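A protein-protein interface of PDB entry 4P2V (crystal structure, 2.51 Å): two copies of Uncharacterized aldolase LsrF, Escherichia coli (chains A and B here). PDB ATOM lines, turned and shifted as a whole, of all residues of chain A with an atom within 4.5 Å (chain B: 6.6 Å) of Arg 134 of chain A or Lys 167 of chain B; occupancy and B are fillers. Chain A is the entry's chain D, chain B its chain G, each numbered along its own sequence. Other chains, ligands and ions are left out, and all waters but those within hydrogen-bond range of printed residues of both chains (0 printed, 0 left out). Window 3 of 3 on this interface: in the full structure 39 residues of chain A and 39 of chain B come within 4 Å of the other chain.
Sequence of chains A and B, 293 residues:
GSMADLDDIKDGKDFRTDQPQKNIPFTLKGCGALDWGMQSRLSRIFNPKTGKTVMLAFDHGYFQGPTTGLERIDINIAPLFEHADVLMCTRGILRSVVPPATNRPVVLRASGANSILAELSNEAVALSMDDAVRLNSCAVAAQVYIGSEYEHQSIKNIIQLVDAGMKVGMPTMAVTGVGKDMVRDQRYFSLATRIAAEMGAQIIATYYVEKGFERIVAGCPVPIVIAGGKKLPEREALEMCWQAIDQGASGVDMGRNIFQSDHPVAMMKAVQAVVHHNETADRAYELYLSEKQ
Among the printed residues, pairs that only touch across the chains: Val 133 of chain A with Val 168 of chain B (3.7 Å), Arg 134 of chain A with Asp 35 of chain B (3.7 Å), Arg 134 of chain A with Gly 37 of chain B (3.1 Å), Arg 134 of chain A with Arg 41 of chain B (3.7 Å), Arg 134 of chain A with Val 168 of chain B (3.1 Å), Leu 135 of chain A with Asp 35 of chain B (3.9 Å), Leu 135 of chain A with Trp 36 of chain B (3.0 Å) and Leu 135 of chain A with Gly 37 of chain B (3.5 Å).
NH2 of Arg 134 of chain A lies within salt-bridge range of OD2 of Asp 130 of chain A, 3.0 Å away. The side-chain carboxylate (OD1) of Asp 131 of chain A is in salt-bridge range of the guanidinium group (NE) of Arg 134 of chain A (3.1 Å). The side-chain carboxylate (OD2) of Asp 35 of chain B lies close to the backbone NH (N) of Gly 37 of chain B (3.3 Å). The guanidinium group of Arg 41 of chain B is in hydrogen-bond range of the backbone carbonyl oxygen of Val 168 of chain B (3.4 Å). The backbone carbonyl oxygen of Gly 169 of chain B sits at hydrogen-bond distance from the guanidinium group of Arg 41 of chain B, at 2.5 Å.
No position is printed for both chains. Of the 11 pairs that touch across the chains among the printed residues, none has its exchanged pair printed and touching as well.
Arg 134 of chain A touches five residues of chain B. Printed residues of chain B within 4 Å of Leu 135 of chain A: Asp 35, Trp 36 and Gly 37. Of the printed residues of chain A, Asp 35 of chain B touches Arg 134 (3.7 Å) and Leu 135 (3.9 Å). Of the printed residues of chain A, Gly 37 of chain B touches Arg 134 (3.1 Å) and Leu 135 (3.5 Å). Printed residues of chain A within 4 Å of Arg 41 of chain B: Val 133 (2.9 Å), Arg 134 (3.7 Å) and Asn 136 (3.4 Å). Of chain A, only Arg 134 comes within 4 Å of Lys 167 of chain B. Printed residues of chain A within 4 Å of Val 168 of chain B: Val 133 and Arg 134. The nearest residue of chain A that does not touch Lys 167 of chain B is Asp 130 of chain A (4.03 Å).
The backbone carbonyl oxygen of Val 133 of chain A lies within hydrogen-bond range of the guanidinium group of Arg 41 of chain B (2.9 Å). The backbone carbonyl oxygen of Lys 167 of chain B lies within hydrogen-bond range of the guanidinium group of Arg 134 of chain A, 2.8 Å away. OD1 of Asn 136 of chain A lies within hydrogen-bond range of NH2 of Arg 41 of chain B, 3.4 Å away.
Of the 7 printed residues of chain A, 4 touch a printed residue of chain B. Printed residues of chain A that touch a printed residue of chain B: Val 133, Arg 134, Leu 135 and Asn 136. Hydrophobic or aromatic side chains of chain B that line the printed part of chain A: Trp 36.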
ATOM      1  N   ASP A 130       9.143 -19.591   8.726  1.00  0.00           N
ATOM      2  CA  ASP A 130       9.865 -20.692   9.349  1.00  0.00           C
ATOM      3  C   ASP A 130       8.949 -21.537  10.232  1.00  0.00           C
ATOM      4  O   ASP A 130       8.973 -22.766  10.171  1.00  0.00           O
ATOM      5  CB  ASP A 130      11.028 -20.138  10.173  1.00  0.00           C
ATOM      6  CG  ASP A 130      11.748 -21.207  10.969  1.00  0.00           C
ATOM      7  OD1 ASP A 130      11.708 -22.392  10.576  1.00  0.00           O
ATOM      8  OD2 ASP A 130      12.351 -20.858  12.004  1.00  0.00           O
ATOM      9  N   ASP A 131       8.131 -20.871  11.041  1.00  0.00           N
ATOM     10  CA  ASP A 131       7.250 -21.571  11.968  1.00  0.00           C
ATOM     11  C   ASP A 131       5.942 -21.992  11.301  1.00  0.00           C
ATOM     12  O   ASP A 131       5.303 -22.951  11.731  1.00  0.00           O
ATOM     13  CB  ASP A 131       6.962 -20.708  13.195  1.00  0.00           C
ATOM     14  CG  ASP A 131       6.669 -21.538  14.428  1.00  0.00           C
ATOM     15  OD1 ASP A 131       7.157 -22.687  14.501  1.00  0.00           O
ATOM     16  OD2 ASP A 131       5.949 -21.048  15.320  1.00  0.00           O
ATOM     17  N   ALA A 132       5.537 -21.261  10.268  1.00  0.00           N
ATOM     18  CA  ALA A 132       4.360 -21.634   9.491  1.00  0.00           C
ATOM     19  C   ALA A 132       4.615 -22.966   8.794  1.00  0.00           C
ATOM     20  O   ALA A 132       3.728 -23.814   8.695  1.00  0.00           O
ATOM     21  CB  ALA A 132       4.016 -20.555   8.479  1.00  0.00           C
ATOM     22  N   VAL A 133       5.839 -23.130   8.302  1.00  0.00           N
ATOM     23  CA  VAL A 133       6.275 -24.379   7.690  1.00  0.00           C
ATOM     24  C   VAL A 133       6.408 -25.526   8.694  1.00  0.00           C
ATOM     25  O   VAL A 133       5.940 -26.637   8.437  1.00  0.00           O
ATOM     26  CB  VAL A 133       7.625 -24.191   6.965  1.00  0.00           C
ATOM     27  CG1 VAL A 133       8.243 -25.536   6.611  1.00  0.00           C
ATOM     28  CG2 VAL A 133       7.447 -23.325   5.727  1.00  0.00           C
ATOM     29  N   ARG A 134       7.033 -25.252   9.837  1.00  0.00           N
ATOM     30  CA  ARG A 134       7.235 -26.272  10.869  1.00  0.00           C
ATOM     31  C   ARG A 134       5.923 -26.911  11.322  1.00  0.00           C
ATOM     32  O   ARG A 134       5.896 -28.078  11.715  1.00  0.00           O
ATOM     33  CB  ARG A 134       7.987 -25.687  12.068  1.00  0.00           C
ATOM     34  CG  ARG A 134       8.276 -26.701  13.171  1.00  0.00           C
ATOM     35  CD  ARG A 134       9.178 -26.129  14.254  1.00  0.00           C
ATOM     36  NE  ARG A 134       9.462 -24.714  14.044  1.00  0.00           N
ATOM     37  CZ  ARG A 134      10.658 -24.235  13.713  1.00  0.00           C
ATOM     38  NH1 ARG A 134      11.686 -25.058  13.553  1.00  0.00           N
ATOM     39  NH2 ARG A 134      10.826 -22.932  13.540  1.00  0.00           N
ATOM     40  N   LEU A 135       4.839 -26.148  11.254  1.00  0.00           N
ATOM     41  CA  LEU A 135       3.539 -26.655  11.668  1.00  0.00           C
ATOM     42  C   LEU A 135       2.761 -27.212  10.476  1.00  0.00           C
ATOM     43  O   LEU A 135       1.593 -27.578  10.608  1.00  0.00           O
ATOM     44  CB  LEU A 135       2.727 -25.557  12.358  1.00  0.00           C
ATOM     45  CG  LEU A 135       3.092 -25.284  13.820  1.00  0.00           C
ATOM     46  CD1 LEU A 135       2.445 -23.993  14.329  1.00  0.00           C
ATOM     47  CD2 LEU A 135       2.754 -26.472  14.705  1.00  0.00           C
ATOM     48  N   ASN A 136       3.419 -27.272   9.320  1.00  0.00           N
ATOM     49  CA  ASN A 136       2.827 -27.821   8.099  1.00  0.00           C
ATOM     50  C   ASN A 136       1.527 -27.112   7.726  1.00  0.00           C
ATOM     51  O   ASN A 136       0.510 -27.751   7.458  1.00  0.00           O
ATOM     52  CB  ASN A 136       2.588 -29.328   8.239  1.00  0.00           C
ATOM     53  CG  ASN A 136       2.229 -29.987   6.918  1.00  0.00           C
ATOM     54  OD1 ASN A 136       2.703 -29.576   5.857  1.00  0.00           O
ATOM     55  ND2 ASN A 136       1.384 -31.007   6.976  1.00  0.00           N
ATOM     56  N   ASP B  35       6.778 -32.316  17.930  1.00  0.00           N
ATOM     57  CA  ASP B  35       6.120 -31.036  17.704  1.00  0.00           C
ATOM     58  C   ASP B  35       4.821 -31.257  16.940  1.00  0.00           C
ATOM     59  O   ASP B  35       4.671 -32.272  16.260  1.00  0.00           O
ATOM     60  CB  ASP B  35       7.047 -30.098  16.924  1.00  0.00           C
ATOM     61  CG  ASP B  35       6.495 -28.693  16.802  1.00  0.00           C
ATOM     62  OD1 ASP B  35       6.483 -27.965  17.816  1.00  0.00           O
ATOM     63  OD2 ASP B  35       6.076 -28.319  15.686  1.00  0.00           O
ATOM     64  N   TRP B  36       3.882 -30.320  17.065  1.00  0.00           N
ATOM     65  CA  TRP B  36       2.587 -30.435  16.399  1.00  0.00           C
ATOM     66  C   TRP B  36       2.724 -30.709  14.908  1.00  0.00           C
ATOM     67  O   TRP B  36       2.091 -31.621  14.379  1.00  0.00           O
ATOM     68  CB  TRP B  36       1.749 -29.170  16.609  1.00  0.00           C
ATOM     69  CG  TRP B  36       0.321 -29.336  16.173  1.00  0.00           C
ATOM     70  CD1 TRP B  36      -0.740 -29.706  16.947  1.00  0.00           C
ATOM     71  CD2 TRP B  36      -0.199 -29.147  14.850  1.00  0.00           C
ATOM     72  NE1 TRP B  36      -1.885 -29.759  16.189  1.00  0.00           N
ATOM     73  CE2 TRP B  36      -1.579 -29.419  14.896  1.00  0.00           C
ATOM     74  CE3 TRP B  36       0.370 -28.771  13.628  1.00  0.00           C
ATOM     75  CZ2 TRP B  36      -2.399 -29.330  13.774  1.00  0.00           C
ATOM     76  CZ3 TRP B  36      -0.445 -28.682  12.516  1.00  0.00           C
ATOM     77  CH2 TRP B  36      -1.814 -28.959  12.595  1.00  0.00           C
ATOM     78  N   GLY B  37       3.562 -29.921  14.242  1.00  0.00           N
ATOM     79  CA  GLY B  37       3.695 -29.996  12.800  1.00  0.00           C
ATOM     80  C   GLY B  37       4.221 -31.333  12.332  1.00  0.00           C
ATOM     81  O   GLY B  37       3.765 -31.874  11.324  1.00  0.00           O
ATOM     82  N   MET B  38       5.187 -31.869  13.067  1.00  0.00           N
ATOM     83  CA  MET B  38       5.722 -33.183  12.756  1.00  0.00           C
ATOM     84  C   MET B  38       4.670 -34.253  13.044  1.00  0.00           C
ATOM     85  O   MET B  38       4.504 -35.192  12.268  1.00  0.00           O
ATOM     86  CB  MET B  38       7.003 -33.447  13.547  1.00  0.00           C
ATOM     87  CG  MET B  38       7.646 -34.787  13.247  1.00  0.00           C
ATOM     88  SD  MET B  38       9.341 -34.888  13.849  1.00  0.00           S
ATOM     89  CE  MET B  38      10.176 -33.813  12.685  1.00  0.00           C
ATOM     90  N   ARG B  41       1.990 -34.107  10.180  1.00  0.00           N
ATOM     91  CA  ARG B  41       2.362 -34.748   8.924  1.00  0.00           C
ATOM     92  C   ARG B  41       2.215 -36.260   9.019  1.00  0.00           C
ATOM     93  O   ARG B  41       1.807 -36.907   8.058  1.00  0.00           O
ATOM     94  CB  ARG B  41       3.793 -34.384   8.526  1.00  0.00           C
ATOM     95  CG  ARG B  41       3.957 -32.949   8.064  1.00  0.00           C
ATOM     96  CD  ARG B  41       5.354 -32.689   7.523  1.00  0.00           C
ATOM     97  NE  ARG B  41       5.455 -31.365   6.915  1.00  0.00           N
ATOM     98  CZ  ARG B  41       5.866 -30.272   7.552  1.00  0.00           C
ATOM     99  NH1 ARG B  41       6.229 -30.337   8.824  1.00  0.00           N
ATOM    100  NH2 ARG B  41       5.917 -29.112   6.910  1.00  0.00           N
ATOM    101  N   VAL B 162      17.368 -36.064   8.635  1.00  0.00           N
ATOM    102  CA  VAL B 162      16.723 -35.821   9.916  1.00  0.00           C
ATOM    103  C   VAL B 162      17.136 -34.450  10.435  1.00  0.00           C
ATOM    104  O   VAL B 162      16.306 -33.685  10.923  1.00  0.00           O
ATOM    105  CB  VAL B 162      17.081 -36.903  10.948  1.00  0.00           C
ATOM    106  CG1 VAL B 162      16.517 -36.547  12.314  1.00  0.00           C
ATOM    107  CG2 VAL B 162      16.571 -38.260  10.492  1.00  0.00           C
ATOM    108  N   ASP B 163      18.421 -34.138  10.297  1.00  0.00           N
ATOM    109  CA  ASP B 163      18.942 -32.830  10.683  1.00  0.00           C
ATOM    110  C   ASP B 163      18.234 -31.711   9.933  1.00  0.00           C
ATOM    111  O   ASP B 163      17.883 -30.691  10.517  1.00  0.00           O
ATOM    112  CB  ASP B 163      20.449 -32.756  10.437  1.00  0.00           C
ATOM    113  CG  ASP B 163      21.249 -33.453  11.518  1.00  0.00           C
ATOM    114  OD1 ASP B 163      20.671 -33.742  12.585  1.00  0.00           O
ATOM    115  OD2 ASP B 163      22.450 -33.716  11.301  1.00  0.00           O
ATOM    116  N   ALA B 164      18.027 -31.905   8.637  1.00  0.00           N
ATOM    117  CA  ALA B 164      17.322 -30.914   7.842  1.00  0.00           C
ATOM    118  C   ALA B 164      15.840 -30.928   8.201  1.00  0.00           C
ATOM    119  O   ALA B 164      15.198 -29.881   8.278  1.00  0.00           O
ATOM    120  CB  ALA B 164      17.521 -31.180   6.363  1.00  0.00           C
ATOM    121  N   GLY B 165      15.306 -32.128   8.410  1.00  0.00           N
ATOM    122  CA  GLY B 165      13.904 -32.303   8.743  1.00  0.00           C
ATOM    123  C   GLY B 165      13.479 -31.773  10.101  1.00  0.00           C
ATOM    124  O   GLY B 165      12.376 -31.247  10.249  1.00  0.00           O
ATOM    125  N   MET B 166      14.356 -31.898  11.095  1.00  0.00           N
ATOM    126  CA  MET B 166      14.028 -31.480  12.457  1.00  0.00           C
ATOM    127  C   MET B 166      13.889 -29.966  12.548  1.00  0.00           C
ATOM    128  O   MET B 166      13.157 -29.445  13.391  1.00  0.00           O
ATOM    129  CB  MET B 166      15.090 -31.975  13.443  1.00  0.00           C
ATOM    130  CG  MET B 166      15.019 -33.470  13.728  1.00  0.00           C
ATOM    131  SD  MET B 166      13.392 -33.985  14.306  1.00  0.00           S
ATOM    132  CE  MET B 166      13.622 -35.753  14.471  1.00  0.00           C
ATOM    133  N   LYS B 167      14.595 -29.270  11.668  1.00  0.00           N
ATOM    134  CA  LYS B 167      14.537 -27.820  11.591  1.00  0.00           C
ATOM    135  C   LYS B 167      13.170 -27.369  11.081  1.00  0.00           C
ATOM    136  O   LYS B 167      12.768 -26.222  11.266  1.00  0.00           O
ATOM    137  CB  LYS B 167      15.652 -27.305  10.680  1.00  0.00           C
ATOM    138  CG  LYS B 167      17.033 -27.708  11.163  1.00  0.00           C
ATOM    139  CD  LYS B 167      18.182 -27.149  10.330  1.00  0.00           C
ATOM    140  CE  LYS B 167      17.781 -25.947   9.498  1.00  0.00           C
ATOM    141  NZ  LYS B 167      18.924 -25.453   8.680  1.00  0.00           N
ATOM    142  N   VAL B 168      12.451 -28.301  10.460  1.00  0.00           N
ATOM    143  CA  VAL B 168      11.300 -27.975   9.628  1.00  0.00           C
ATOM    144  C   VAL B 168      10.053 -28.811   9.956  1.00  0.00           C
ATOM    145  O   VAL B 168       8.938 -28.486   9.540  1.00  0.00           O
ATOM    146  CB  VAL B 168      11.712 -28.148   8.126  1.00  0.00           C
ATOM    147  CG1 VAL B 168      10.647 -28.826   7.267  1.00  0.00           C
ATOM    148  CG2 VAL B 168      12.244 -26.837   7.542  1.00  0.00           C
ATOM    149  N   GLY B 169      10.227 -29.850  10.760  1.00  0.00           N
ATOM    150  CA  GLY B 169       9.100 -30.672  11.157  1.00  0.00           C
ATOM    151  C   GLY B 169       8.764 -31.672  10.071  1.00  0.00           C
ATOM    152  O   GLY B 169       7.615 -32.089   9.931  1.00  0.00           O
ATOM    153  N   MET B 170       9.773 -32.044   9.289  1.00  0.00           N
ATOM    154  CA  MET B 170       9.595 -32.984   8.187  1.00  0.00           C
ATOM    155  C   MET B 170      10.116 -34.365   8.564  1.00  0.00           C
ATOM    156  O   MET B 170      11.309 -34.538   8.807  1.00  0.00           O
ATOM    157  CB  MET B 170      10.300 -32.485   6.923  1.00  0.00           C
ATOM    158  CG  MET B 170      10.135 -33.409   5.725  1.00  0.00           C
ATOM    159  SD  MET B 170       8.480 -33.385   5.003  1.00  0.00           S
ATOM    160  CE  MET B 170       8.433 -31.737   4.304  1.00  0.00           C
